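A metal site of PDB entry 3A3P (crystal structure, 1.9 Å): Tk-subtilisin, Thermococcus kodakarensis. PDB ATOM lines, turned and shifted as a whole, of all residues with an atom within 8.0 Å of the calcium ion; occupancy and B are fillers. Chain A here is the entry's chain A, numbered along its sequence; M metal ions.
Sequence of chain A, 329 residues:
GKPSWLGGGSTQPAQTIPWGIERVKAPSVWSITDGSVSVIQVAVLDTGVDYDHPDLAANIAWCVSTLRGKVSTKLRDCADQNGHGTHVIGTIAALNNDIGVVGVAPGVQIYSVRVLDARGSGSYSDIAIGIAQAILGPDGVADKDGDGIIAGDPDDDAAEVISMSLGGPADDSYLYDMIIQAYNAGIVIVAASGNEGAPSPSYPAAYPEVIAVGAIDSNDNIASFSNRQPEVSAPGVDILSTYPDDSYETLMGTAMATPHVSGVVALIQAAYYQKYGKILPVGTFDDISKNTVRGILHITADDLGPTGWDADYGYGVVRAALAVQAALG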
ATOM      1  N   GLN A  12     -20.656 -39.869 -18.647  1.00  0.00           N
ATOM      2  CA  GLN A  12     -21.230 -38.467 -18.516  1.00  0.00           C
ATOM      3  C   GLN A  12     -22.730 -38.400 -18.789  1.00  0.00           C
ATOM      4  O   GLN A  12     -23.196 -38.963 -19.772  1.00  0.00           O
ATOM      5  CB  GLN A  12     -20.498 -37.488 -19.446  1.00  0.00           C
ATOM      6  CG  GLN A  12     -19.049 -37.238 -19.065  1.00  0.00           C
ATOM      7  CD  GLN A  12     -18.940 -36.379 -17.821  1.00  0.00           C
ATOM      8  OE1 GLN A  12     -19.631 -35.357 -17.686  1.00  0.00           O
ATOM      9  NE2 GLN A  12     -18.071 -36.782 -16.914  1.00  0.00           N
ATOM     10  N   PRO A  13     -23.479 -37.694 -17.919  1.00  0.00           N
ATOM     11  CA  PRO A  13     -24.929 -37.524 -18.113  1.00  0.00           C
ATOM     12  C   PRO A  13     -25.234 -36.557 -19.270  1.00  0.00           C
ATOM     13  O   PRO A  13     -24.436 -35.657 -19.527  1.00  0.00           O
ATOM     14  CB  PRO A  13     -25.407 -36.932 -16.775  1.00  0.00           C
ATOM     15  CG  PRO A  13     -24.211 -36.209 -16.252  1.00  0.00           C
ATOM     16  CD  PRO A  13     -23.006 -37.030 -16.692  1.00  0.00           C
ATOM     17  N   ALA A  14     -26.367 -36.741 -19.965  1.00  0.00           N
ATOM     18  CA  ALA A  14     -26.845 -35.779 -20.951  1.00  0.00           C
ATOM     19  C   ALA A  14     -26.990 -34.373 -20.335  1.00  0.00           C
ATOM     20  O   ALA A  14     -27.278 -34.255 -19.162  1.00  0.00           O
ATOM     21  CB  ALA A  14     -28.211 -36.238 -21.503  1.00  0.00           C
ATOM     22  N   GLN A  15     -26.818 -33.336 -21.142  1.00  0.00           N
ATOM     23  CA  GLN A  15     -26.785 -31.969 -20.622  1.00  0.00           C
ATOM     24  C   GLN A  15     -28.143 -31.486 -20.151  1.00  0.00           C
ATOM     25  O   GLN A  15     -29.135 -31.727 -20.844  1.00  0.00           O
ATOM     26  CB  GLN A  15     -26.214 -31.007 -21.659  1.00  0.00           C
ATOM     27  CG  GLN A  15     -26.243 -29.533 -21.205  1.00  0.00           C
ATOM     28  CD  GLN A  15     -25.519 -28.624 -22.152  1.00  0.00           C
ATOM     29  OE1 GLN A  15     -24.289 -28.552 -22.134  1.00  0.00           O
ATOM     30  NE2 GLN A  15     -26.267 -27.915 -22.982  1.00  0.00           N
ATOM     31  N   THR A  16     -28.182 -30.834 -18.991  1.00  0.00           N
ATOM     32  CA  THR A  16     -29.321 -29.996 -18.586  1.00  0.00           C
ATOM     33  C   THR A  16     -28.944 -28.562 -18.374  1.00  0.00           C
ATOM     34  O   THR A  16     -27.779 -28.267 -18.089  1.00  0.00           O
ATOM     35  CB  THR A  16     -29.913 -30.293 -17.166  1.00  0.00           C
ATOM     36  OG1 THR A  16     -28.993 -31.022 -16.322  1.00  0.00           O
ATOM     37  CG2 THR A  16     -31.232 -30.887 -17.239  1.00  0.00           C
ATOM     38  N   HIS A  53     -11.936 -31.604 -16.055  1.00  0.00           N
ATOM     39  CA  HIS A  53     -13.357 -31.882 -16.131  1.00  0.00           C
ATOM     40  C   HIS A  53     -13.836 -31.754 -17.570  1.00  0.00           C
ATOM     41  O   HIS A  53     -13.677 -30.705 -18.181  1.00  0.00           O
ATOM     42  CB  HIS A  53     -14.193 -30.951 -15.214  1.00  0.00           C
ATOM     43  CG  HIS A  53     -15.614 -31.407 -15.070  1.00  0.00           C
ATOM     44  ND1 HIS A  53     -16.171 -31.792 -13.868  1.00  0.00           N
ATOM     45  CD2 HIS A  53     -16.591 -31.580 -15.994  1.00  0.00           C
ATOM     46  CE1 HIS A  53     -17.432 -32.142 -14.046  1.00  0.00           C
ATOM     47  NE2 HIS A  53     -17.710 -32.036 -15.326  1.00  0.00           N
ATOM     48  N   PRO A  54     -14.478 -32.811 -18.112  1.00  0.00           N
ATOM     49  CA  PRO A  54     -14.947 -32.780 -19.489  1.00  0.00           C
ATOM     50  C   PRO A  54     -15.868 -31.580 -19.802  1.00  0.00           C
ATOM     51  O   PRO A  54     -15.920 -31.118 -20.954  1.00  0.00           O
ATOM     52  CB  PRO A  54     -15.709 -34.103 -19.638  1.00  0.00           C
ATOM     53  CG  PRO A  54     -15.116 -35.038 -18.621  1.00  0.00           C
ATOM     54  CD  PRO A  54     -14.773 -34.102 -17.444  1.00  0.00           C
ATOM     55  N   ASP A  55     -16.568 -31.052 -18.810  1.00  0.00           N
ATOM     56  CA  ASP A  55     -17.508 -29.957 -19.080  1.00  0.00           C
ATOM     57  C   ASP A  55     -16.936 -28.578 -18.779  1.00  0.00           C
ATOM     58  O   ASP A  55     -17.655 -27.561 -18.826  1.00  0.00           O
ATOM     59  CB  ASP A  55     -18.831 -30.187 -18.320  1.00  0.00           C
ATOM     60  CG  ASP A  55     -20.039 -29.755 -19.120  1.00  0.00           C
ATOM     61  OD1 ASP A  55     -19.975 -29.754 -20.368  1.00  0.00           O
ATOM     62  OD2 ASP A  55     -21.071 -29.419 -18.521  1.00  0.00           O
ATOM     63  N   LEU A  56     -15.638 -28.555 -18.469  1.00  0.00           N
ATOM     64  CA  LEU A  56     -14.923 -27.328 -18.120  1.00  0.00           C
ATOM     65  C   LEU A  56     -13.634 -27.098 -18.895  1.00  0.00           C
ATOM     66  O   LEU A  56     -13.257 -25.942 -19.152  1.00  0.00           O
ATOM     67  CB  LEU A  56     -14.559 -27.334 -16.633  1.00  0.00           C
ATOM     68  CG  LEU A  56     -15.646 -27.380 -15.554  1.00  0.00           C
ATOM     69  CD1 LEU A  56     -14.916 -27.187 -14.227  1.00  0.00           C
ATOM     70  CD2 LEU A  56     -16.696 -26.272 -15.746  1.00  0.00           C
ATOM     71  N   ALA A  93     -19.151 -21.035 -16.508  1.00  0.00           N
ATOM     72  CA  ALA A  93     -18.533 -21.381 -17.799  1.00  0.00           C
ATOM     73  C   ALA A  93     -18.577 -22.849 -18.198  1.00  0.00           C
ATOM     74  O   ALA A  93     -17.802 -23.250 -19.076  1.00  0.00           O
ATOM     75  CB  ALA A  93     -17.078 -20.869 -17.863  1.00  0.00           C
ATOM     76  N   ALA A  94     -19.471 -23.651 -17.604  1.00  0.00           N
ATOM     77  CA  ALA A  94     -19.627 -25.043 -18.113  1.00  0.00           C
ATOM     78  C   ALA A  94     -20.037 -24.986 -19.579  1.00  0.00           C
ATOM     79  O   ALA A  94     -20.825 -24.149 -19.961  1.00  0.00           O
ATOM     80  CB  ALA A  94     -20.665 -25.857 -17.297  1.00  0.00           C
ATOM     81  N   LEU A  95     -19.461 -25.853 -20.394  1.00  0.00           N
ATOM     82  CA  LEU A  95     -19.576 -25.762 -21.841  1.00  0.00           C
ATOM     83  C   LEU A  95     -20.990 -26.133 -22.294  1.00  0.00           C
ATOM     84  O   LEU A  95     -21.655 -26.953 -21.648  1.00  0.00           O
ATOM     85  CB  LEU A  95     -18.540 -26.726 -22.447  1.00  0.00           C
ATOM     86  CG  LEU A  95     -17.098 -26.267 -22.254  1.00  0.00           C
ATOM     87  CD1 LEU A  95     -16.104 -27.462 -22.181  1.00  0.00           C
ATOM     88  CD2 LEU A  95     -16.730 -25.306 -23.348  1.00  0.00           C
ATOM     89  N   ASN A  96     -21.433 -25.537 -23.386  1.00  0.00           N
ATOM     90  CA  ASN A  96     -22.719 -25.851 -23.988  1.00  0.00           C
ATOM     91  C   ASN A  96     -22.448 -26.942 -25.018  1.00  0.00           C
ATOM     92  O   ASN A  96     -21.957 -26.662 -26.103  1.00  0.00           O
ATOM     93  CB  ASN A  96     -23.280 -24.621 -24.668  1.00  0.00           C
ATOM     94  CG  ASN A  96     -24.727 -24.783 -25.155  1.00  0.00           C
ATOM     95  OD1 ASN A  96     -25.340 -25.826 -24.978  1.00  0.00           O
ATOM     96  ND2 ASN A  96     -25.252 -23.749 -25.744  1.00  0.00           N
ATOM     97  N   ASN A  97     -22.755 -28.173 -24.649  1.00  0.00           N
ATOM     98  CA  ASN A  97     -22.375 -29.363 -25.442  1.00  0.00           C
ATOM     99  C   ASN A  97     -23.422 -30.444 -25.181  1.00  0.00           C
ATOM    100  O   ASN A  97     -24.574 -30.120 -24.887  1.00  0.00           O
ATOM    101  CB  ASN A  97     -20.948 -29.850 -25.080  1.00  0.00           C
ATOM    102  CG  ASN A  97     -20.738 -30.056 -23.565  1.00  0.00           C
ATOM    103  OD1 ASN A  97     -21.683 -30.195 -22.803  1.00  0.00           O
ATOM    104  ND2 ASN A  97     -19.477 -30.108 -23.140  1.00  0.00           N
ATOM    105  N   ASP A  98     -23.036 -31.710 -25.220  1.00  0.00           N
ATOM    106  CA  ASP A  98     -24.017 -32.754 -24.958  1.00  0.00           C
ATOM    107  C   ASP A  98     -24.044 -33.371 -23.572  1.00  0.00           C
ATOM    108  O   ASP A  98     -24.807 -34.307 -23.328  1.00  0.00           O
ATOM    109  CB  ASP A  98     -23.994 -33.793 -26.081  1.00  0.00           C
ATOM    110  CG  ASP A  98     -24.415 -33.181 -27.418  1.00  0.00           C
ATOM    111  OD1 ASP A  98     -25.642 -32.903 -27.622  1.00  0.00           O
ATOM    112  OD2 ASP A  98     -23.514 -32.916 -28.265  1.00  0.00           O
ATOM    113  N   ILE A  99     -23.238 -32.839 -22.639  1.00  0.00           N
ATOM    114  CA  ILE A  99     -23.113 -33.428 -21.314  1.00  0.00           C
ATOM    115  C   ILE A  99     -23.291 -32.416 -20.162  1.00  0.00           C
ATOM    116  O   ILE A  99     -23.147 -31.208 -20.335  1.00  0.00           O
ATOM    117  CB  ILE A  99     -21.701 -34.095 -21.142  1.00  0.00           C
ATOM    118  CG1 ILE A  99     -20.598 -33.068 -21.431  1.00  0.00           C
ATOM    119  CG2 ILE A  99     -21.525 -35.290 -22.144  1.00  0.00           C
ATOM    120  CD1 ILE A  99     -19.265 -33.397 -20.830  1.00  0.00           C
ATOM    121  N   GLY A 100     -23.560 -32.937 -18.983  1.00  0.00           N
ATOM    122  CA  GLY A 100     -23.417 -32.179 -17.750  1.00  0.00           C
ATOM    123  C   GLY A 100     -24.353 -31.000 -17.638  1.00  0.00           C
ATOM    124  O   GLY A 100     -25.582 -31.136 -17.677  1.00  0.00           O
ATOM    125  N   VAL A 101     -23.775 -29.829 -17.415  1.00  0.00           N
ATOM    126  CA  VAL A 101     -24.586 -28.626 -17.256  1.00  0.00           C
ATOM    127  C   VAL A 101     -24.192 -27.577 -18.294  1.00  0.00           C
ATOM    128  O   VAL A 101     -23.606 -27.923 -19.335  1.00  0.00           O
ATOM    129  CB  VAL A 101     -24.481 -28.088 -15.810  1.00  0.00           C
ATOM    130  CG1 VAL A 101     -25.131 -29.084 -14.825  1.00  0.00           C
ATOM    131  CG2 VAL A 101     -23.014 -27.812 -15.436  1.00  0.00           C
ATOM    132  N   VAL A 102     -24.502 -26.295 -18.065  1.00  0.00           N
ATOM    133  CA  VAL A 102     -24.067 -25.228 -18.985  1.00  0.00           C
ATOM    134  C   VAL A 102     -23.963 -23.963 -18.137  1.00  0.00           C
ATOM    135  O   VAL A 102     -24.793 -23.745 -17.253  1.00  0.00           O
ATOM    136  CB  VAL A 102     -24.989 -25.059 -20.255  1.00  0.00           C
ATOM    137  CG1 VAL A 102     -26.481 -24.820 -19.903  1.00  0.00           C
ATOM    138  CG2 VAL A 102     -24.500 -23.944 -21.211  1.00  0.00           C
ATOM    139  N   GLY A 103     -22.900 -23.167 -18.353  1.00  0.00           N
ATOM    140  CA  GLY A 103     -22.752 -21.982 -17.518  1.00  0.00           C
ATOM    141  C   GLY A 103     -23.523 -20.813 -18.085  1.00  0.00           C
ATOM    142  O   GLY A 103     -24.050 -20.907 -19.189  1.00  0.00           O
ATOM    143  N   PRO A 106     -21.179 -19.826 -21.440  1.00  0.00           N
ATOM    144  CA  PRO A 106     -20.559 -21.127 -21.677  1.00  0.00           C
ATOM    145  C   PRO A 106     -19.323 -21.136 -22.617  1.00  0.00           C
ATOM    146  O   PRO A 106     -18.691 -22.202 -22.782  1.00  0.00           O
ATOM    147  CB  PRO A 106     -21.726 -21.963 -22.268  1.00  0.00           C
ATOM    148  CG  PRO A 106     -22.674 -21.019 -22.810  1.00  0.00           C
ATOM    149  CD  PRO A 106     -22.518 -19.705 -22.055  1.00  0.00           C
ATOM    150  N   THR A 242     -20.827 -28.385 -11.929  1.00  0.00           N
ATOM    151  CA  THR A 242     -19.719 -29.326 -11.968  1.00  0.00           C
ATOM    152  C   THR A 242     -19.086 -29.512 -10.591  1.00  0.00           C
ATOM    153  O   THR A 242     -19.100 -28.620  -9.726  1.00  0.00           O
ATOM    154  CB  THR A 242     -18.648 -28.831 -12.964  1.00  0.00           C
ATOM    155  OG1 THR A 242     -18.439 -27.413 -12.761  1.00  0.00           O
ATOM    156  CG2 THR A 242     -19.120 -29.050 -14.420  1.00  0.00           C
ATOM    157  N   TYR A 248     -20.842 -33.952 -10.873  1.00  0.00           N
ATOM    158  CA  TYR A 248     -21.797 -32.829 -10.664  1.00  0.00           C
ATOM    159  C   TYR A 248     -22.367 -32.935  -9.253  1.00  0.00           C
ATOM    160  O   TYR A 248     -22.458 -34.025  -8.711  1.00  0.00           O
ATOM    161  CB  TYR A 248     -22.914 -32.871 -11.722  1.00  0.00           C
ATOM    162  CG  TYR A 248     -22.333 -32.962 -13.097  1.00  0.00           C
ATOM    163  CD1 TYR A 248     -21.989 -34.208 -13.655  1.00  0.00           C
ATOM    164  CD2 TYR A 248     -22.040 -31.815 -13.807  1.00  0.00           C
ATOM    165  CE1 TYR A 248     -21.386 -34.285 -14.901  1.00  0.00           C
ATOM    166  CE2 TYR A 248     -21.445 -31.876 -15.045  1.00  0.00           C
ATOM    167  CZ  TYR A 248     -21.109 -33.120 -15.587  1.00  0.00           C
ATOM    168  OH  TYR A 248     -20.507 -33.147 -16.837  1.00  0.00           O
HETATM  169 CA    CA M   1     -22.275 -29.062 -20.824  1.00  0.00          CA
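Of the 23 residues printed, 6 come within 4 Å of the calcium ion.
O of Val 101 is bound to the calcium ion. The calcium ion is bound by O of Leu 95 (2.3 Å). The side-chain amide oxygen (OD1) of Asn 97 is bound to the calcium ion, 2.4 Å away. The calcium ion is bound by O of Ile 99, 2.4 Å away. The side-chain carboxylate (OD1) of Asp 55 binds the calcium ion. OE1 of Gln 15 binds the calcium ion (2.5 Å). OD2 of Asp 55 is bound to the calcium ion, at 2.6 Å.
The side-chain amide nitrogen (NE2) of Gln 15 is in hydrogen-bond range of the side-chain amide oxygen (OD1) of Asn 96, at 3.0 Å. The backbone NH of Gln 15 lies within hydrogen-bond range of the backbone carbonyl oxygen of Asp 98 (3.1 Å).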
